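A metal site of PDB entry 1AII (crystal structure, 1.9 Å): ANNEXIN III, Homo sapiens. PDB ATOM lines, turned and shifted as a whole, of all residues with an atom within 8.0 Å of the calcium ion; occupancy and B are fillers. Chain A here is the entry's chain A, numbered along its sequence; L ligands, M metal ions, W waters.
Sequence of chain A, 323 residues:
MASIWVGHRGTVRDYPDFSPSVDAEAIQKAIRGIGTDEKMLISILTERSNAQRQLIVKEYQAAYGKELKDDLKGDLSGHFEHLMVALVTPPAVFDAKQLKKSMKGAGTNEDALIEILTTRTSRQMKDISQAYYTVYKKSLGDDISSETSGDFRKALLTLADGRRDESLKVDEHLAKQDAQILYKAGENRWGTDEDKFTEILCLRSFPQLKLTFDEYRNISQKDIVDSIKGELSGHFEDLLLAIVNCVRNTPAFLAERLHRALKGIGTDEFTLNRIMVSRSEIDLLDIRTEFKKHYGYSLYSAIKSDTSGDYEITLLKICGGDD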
ATOM      1  N   LEU A 182       9.323  -5.002  14.481  1.00  0.00           N
ATOM      2  CA  LEU A 182      10.493  -4.599  13.687  1.00  0.00           C
ATOM      3  C   LEU A 182      11.759  -4.899  14.500  1.00  0.00           C
ATOM      4  O   LEU A 182      12.771  -5.398  14.023  1.00  0.00           O
ATOM      5  CB  LEU A 182      10.438  -3.118  13.322  1.00  0.00           C
ATOM      6  CG  LEU A 182       9.496  -2.644  12.194  1.00  0.00           C
ATOM      7  CD1 LEU A 182       9.629  -1.142  11.973  1.00  0.00           C
ATOM      8  CD2 LEU A 182       9.748  -3.399  10.898  1.00  0.00           C
ATOM      9  N   TYR A 183      11.725  -4.547  15.778  1.00  0.00           N
ATOM     10  CA  TYR A 183      12.842  -4.764  16.694  1.00  0.00           C
ATOM     11  C   TYR A 183      13.172  -6.254  16.788  1.00  0.00           C
ATOM     12  O   TYR A 183      14.351  -6.614  16.710  1.00  0.00           O
ATOM     13  CB  TYR A 183      12.576  -4.193  18.083  1.00  0.00           C
ATOM     14  CG  TYR A 183      13.751  -4.283  19.026  1.00  0.00           C
ATOM     15  CD1 TYR A 183      14.863  -3.453  18.867  1.00  0.00           C
ATOM     16  CD2 TYR A 183      13.762  -5.177  20.088  1.00  0.00           C
ATOM     17  CE1 TYR A 183      15.933  -3.523  19.729  1.00  0.00           C
ATOM     18  CE2 TYR A 183      14.842  -5.266  20.955  1.00  0.00           C
ATOM     19  CZ  TYR A 183      15.932  -4.437  20.773  1.00  0.00           C
ATOM     20  OH  TYR A 183      17.008  -4.526  21.631  1.00  0.00           O
ATOM     21  N   LYS A 184      12.202  -7.127  16.940  1.00  0.00           N
ATOM     22  CA  LYS A 184      12.396  -8.562  17.038  1.00  0.00           C
ATOM     23  C   LYS A 184      12.864  -9.154  15.715  1.00  0.00           C
ATOM     24  O   LYS A 184      13.602 -10.137  15.727  1.00  0.00           O
ATOM     25  CB  LYS A 184      11.115  -9.320  17.422  1.00  0.00           C
ATOM     26  CG  LYS A 184      10.691  -9.147  18.867  1.00  0.00           C
ATOM     27  CD  LYS A 184       9.506 -10.037  19.247  1.00  0.00           C
ATOM     28  CE  LYS A 184       8.824  -9.500  20.493  1.00  0.00           C
ATOM     29  NZ  LYS A 184       7.380  -9.888  20.584  1.00  0.00           N
ATOM     30  N   ALA A 185      12.423  -8.563  14.606  1.00  0.00           N
ATOM     31  CA  ALA A 185      12.767  -9.019  13.278  1.00  0.00           C
ATOM     32  C   ALA A 185      14.173  -8.702  12.796  1.00  0.00           C
ATOM     33  O   ALA A 185      14.677  -9.317  11.857  1.00  0.00           O
ATOM     34  CB  ALA A 185      11.786  -8.342  12.287  1.00  0.00           C
ATOM     35  N   GLY A 186      14.804  -7.739  13.425  1.00  0.00           N
ATOM     36  CA  GLY A 186      16.121  -7.271  13.101  1.00  0.00           C
ATOM     37  C   GLY A 186      17.053  -7.197  14.289  1.00  0.00           C
ATOM     38  O   GLY A 186      17.662  -8.202  14.609  1.00  0.00           O
ATOM     39  N   GLU A 187      17.214  -6.103  14.972  1.00  0.00           N
ATOM     40  CA  GLU A 187      18.100  -5.931  16.091  1.00  0.00           C
ATOM     41  C   GLU A 187      18.141  -7.060  17.097  1.00  0.00           C
ATOM     42  O   GLU A 187      19.227  -7.465  17.487  1.00  0.00           O
ATOM     43  CB  GLU A 187      17.753  -4.642  16.874  1.00  0.00           C
ATOM     44  CG  GLU A 187      17.964  -3.381  16.067  1.00  0.00           C
ATOM     45  CD  GLU A 187      19.415  -3.010  15.825  1.00  0.00           C
ATOM     46  OE1 GLU A 187      20.354  -3.586  16.408  1.00  0.00           O
ATOM     47  OE2 GLU A 187      19.677  -2.091  15.043  1.00  0.00           O
ATOM     48  N   ASN A 188      16.989  -7.539  17.540  1.00  0.00           N
ATOM     49  CA  ASN A 188      16.934  -8.585  18.533  1.00  0.00           C
ATOM     50  C   ASN A 188      17.242  -9.995  18.095  1.00  0.00           C
ATOM     51  O   ASN A 188      17.210 -10.872  18.979  1.00  0.00           O
ATOM     52  CB  ASN A 188      15.530  -8.533  19.179  1.00  0.00           C
ATOM     53  CG  ASN A 188      15.534  -9.105  20.596  1.00  0.00           C
ATOM     54  OD1 ASN A 188      14.796 -10.062  20.850  1.00  0.00           O
ATOM     55  ND2 ASN A 188      16.359  -8.533  21.465  1.00  0.00           N
ATOM     56  N   ARG A 189      17.539 -10.314  16.858  1.00  0.00           N
ATOM     57  CA  ARG A 189      17.826 -11.717  16.554  1.00  0.00           C
ATOM     58  C   ARG A 189      19.050 -11.890  15.697  1.00  0.00           C
ATOM     59  O   ARG A 189      19.489 -10.882  15.171  1.00  0.00           O
ATOM     60  CB  ARG A 189      16.640 -12.305  15.774  1.00  0.00           C
ATOM     61  CG  ARG A 189      16.227 -11.509  14.544  1.00  0.00           C
ATOM     62  CD  ARG A 189      15.329 -12.354  13.667  1.00  0.00           C
ATOM     63  NE  ARG A 189      16.106 -13.254  12.826  1.00  0.00           N
ATOM     64  CZ  ARG A 189      15.648 -14.150  11.972  1.00  0.00           C
ATOM     65  NH1 ARG A 189      14.339 -14.324  11.801  1.00  0.00           N
ATOM     66  NH2 ARG A 189      16.489 -14.901  11.268  1.00  0.00           N
ATOM     67  N   TRP A 190      19.588 -13.083  15.533  1.00  0.00           N
ATOM     68  CA  TRP A 190      20.743 -13.273  14.664  1.00  0.00           C
ATOM     69  C   TRP A 190      20.133 -13.183  13.250  1.00  0.00           C
ATOM     70  O   TRP A 190      19.038 -13.727  13.055  1.00  0.00           O
ATOM     71  CB  TRP A 190      21.422 -14.634  14.863  1.00  0.00           C
ATOM     72  CG  TRP A 190      22.070 -14.783  16.208  1.00  0.00           C
ATOM     73  CD1 TRP A 190      22.413 -13.807  17.082  1.00  0.00           C
ATOM     74  CD2 TRP A 190      22.460 -16.021  16.819  1.00  0.00           C
ATOM     75  NE1 TRP A 190      22.969 -14.347  18.205  1.00  0.00           N
ATOM     76  CE2 TRP A 190      23.009 -15.707  18.061  1.00  0.00           C
ATOM     77  CE3 TRP A 190      22.368 -17.359  16.407  1.00  0.00           C
ATOM     78  CZ2 TRP A 190      23.496 -16.682  18.948  1.00  0.00           C
ATOM     79  CZ3 TRP A 190      22.851 -18.320  17.274  1.00  0.00           C
ATOM     80  CH2 TRP A 190      23.412 -17.980  18.513  1.00  0.00           C
ATOM     81  N   GLY A 191      20.800 -12.541  12.277  1.00  0.00           N
ATOM     82  CA  GLY A 191      20.111 -12.473  11.002  1.00  0.00           C
ATOM     83  C   GLY A 191      18.979 -11.477  11.008  1.00  0.00           C
ATOM     84  O   GLY A 191      18.878 -10.632  11.901  1.00  0.00           O
ATOM     85  N   THR A 192      18.100 -11.561  10.027  1.00  0.00           N
ATOM     86  CA  THR A 192      16.976 -10.647   9.933  1.00  0.00           C
ATOM     87  C   THR A 192      15.752 -11.289   9.301  1.00  0.00           C
ATOM     88  O   THR A 192      15.884 -12.112   8.395  1.00  0.00           O
ATOM     89  CB  THR A 192      17.329  -9.414   9.054  1.00  0.00           C
ATOM     90  OG1 THR A 192      18.594  -8.897   9.442  1.00  0.00           O
ATOM     91  CG2 THR A 192      16.254  -8.342   9.172  1.00  0.00           C
ATOM     92  N   ASP A 193      14.575 -10.957   9.790  1.00  0.00           N
ATOM     93  CA  ASP A 193      13.362 -11.433   9.144  1.00  0.00           C
ATOM     94  C   ASP A 193      12.945 -10.386   8.117  1.00  0.00           C
ATOM     95  O   ASP A 193      12.033  -9.605   8.366  1.00  0.00           O
ATOM     96  CB  ASP A 193      12.252 -11.722  10.164  1.00  0.00           C
ATOM     97  CG  ASP A 193      11.038 -12.366   9.505  1.00  0.00           C
ATOM     98  OD1 ASP A 193      10.992 -12.395   8.249  1.00  0.00           O
ATOM     99  OD2 ASP A 193      10.138 -12.826  10.227  1.00  0.00           O
ATOM    100  N   PHE A 197      10.096  -6.844   7.586  1.00  0.00           N
ATOM    101  CA  PHE A 197      10.460  -5.461   7.284  1.00  0.00           C
ATOM    102  C   PHE A 197       9.630  -5.011   6.076  1.00  0.00           C
ATOM    103  O   PHE A 197       9.045  -3.941   6.064  1.00  0.00           O
ATOM    104  CB  PHE A 197      11.957  -5.273   7.015  1.00  0.00           C
ATOM    105  CG  PHE A 197      12.764  -4.970   8.252  1.00  0.00           C
ATOM    106  CD1 PHE A 197      13.171  -5.973   9.120  1.00  0.00           C
ATOM    107  CD2 PHE A 197      13.105  -3.658   8.572  1.00  0.00           C
ATOM    108  CE1 PHE A 197      13.910  -5.654  10.246  1.00  0.00           C
ATOM    109  CE2 PHE A 197      13.835  -3.342   9.702  1.00  0.00           C
ATOM    110  CZ  PHE A 197      14.241  -4.341  10.548  1.00  0.00           C
ATOM    111  N   SER A 227      18.960   0.820  12.057  1.00  0.00           N
ATOM    112  CA  SER A 227      18.708  -0.622  12.097  1.00  0.00           C
ATOM    113  C   SER A 227      18.705  -1.189  10.685  1.00  0.00           C
ATOM    114  O   SER A 227      19.235  -2.266  10.423  1.00  0.00           O
ATOM    115  CB  SER A 227      17.417  -0.962  12.833  1.00  0.00           C
ATOM    116  OG  SER A 227      17.486  -0.611  14.205  1.00  0.00           O
ATOM    117  N   GLY A 230      22.147  -1.433   9.638  1.00  0.00           N
ATOM    118  CA  GLY A 230      23.011  -2.459  10.188  1.00  0.00           C
ATOM    119  C   GLY A 230      22.515  -3.853   9.893  1.00  0.00           C
ATOM    120  O   GLY A 230      23.275  -4.827   9.984  1.00  0.00           O
ATOM    121  N   GLU A 231      21.242  -3.972   9.520  1.00  0.00           N
ATOM    122  CA  GLU A 231      20.626  -5.271   9.270  1.00  0.00           C
ATOM    123  C   GLU A 231      20.613  -5.692   7.809  1.00  0.00           C
ATOM    124  O   GLU A 231      20.808  -6.861   7.481  1.00  0.00           O
ATOM    125  CB  GLU A 231      19.170  -5.287   9.723  1.00  0.00           C
ATOM    126  CG  GLU A 231      18.985  -5.163  11.214  1.00  0.00           C
ATOM    127  CD  GLU A 231      19.372  -6.429  11.947  1.00  0.00           C
ATOM    128  OE1 GLU A 231      19.007  -7.523  11.478  1.00  0.00           O
ATOM    129  OE2 GLU A 231      20.052  -6.321  12.995  1.00  0.00           O
ATOM    130  N   LEU A 232      20.368  -4.752   6.911  1.00  0.00           N
ATOM    131  CA  LEU A 232      20.245  -5.099   5.499  1.00  0.00           C
ATOM    132  C   LEU A 232      21.366  -4.498   4.667  1.00  0.00           C
ATOM    133  O   LEU A 232      22.227  -3.792   5.171  1.00  0.00           O
ATOM    134  CB  LEU A 232      18.864  -4.672   5.023  1.00  0.00           C
ATOM    135  CG  LEU A 232      17.708  -4.953   5.999  1.00  0.00           C
ATOM    136  CD1 LEU A 232      16.577  -3.947   5.815  1.00  0.00           C
ATOM    137  CD2 LEU A 232      17.198  -6.369   5.833  1.00  0.00           C
HETATM  138  C1  LIG L   1      19.894 -14.122   8.353  1.00  0.00           C
HETATM  139  N1  LIG L   1      19.263 -15.351   8.912  1.00  0.00           N
HETATM  140  C2  LIG L   1      21.249 -14.411   7.757  1.00  0.00           C
HETATM  141  O1  LIG L   1      21.359 -15.803   7.509  1.00  0.00           O
HETATM  142 CA    CA M   1      19.844  -9.039  13.423  1.00  0.00          CA
HETATM  143  O   HOH W   1      21.244  -8.280  15.611  1.00  0.00           O
HETATM  144  O   HOH W   2      22.079  -9.402  11.991  1.00  0.00           O
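Within 4 Å of the calcium ion: Gly 186, Arg 189, Gly 191 and Glu 231.
The side-chain carboxylate (OE1) of Glu 231 lies close to the side-chain hydroxyl (OG1) of Thr 192 (2.5 Å). The side-chain carboxylate (OE2) of Glu 231 lies close to the backbone NH (N) of Glu 187 (3.5 Å).
The calcium ion is bound by the backbone carbonyl oxygen (O) of Gly 191 (2.4 Å), the backbone carbonyl oxygen (O) of Arg 189 (2.6 Å), the side-chain carboxylate (OE1) of Glu 231 (2.6 Å), the backbone carbonyl oxygen (O) of Gly 186 (2.6 Å), water W2 (2.7 Å), water W1 (2.7 Å) and the side-chain carboxylate (OE2) of Glu 231 (2.8 Å).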
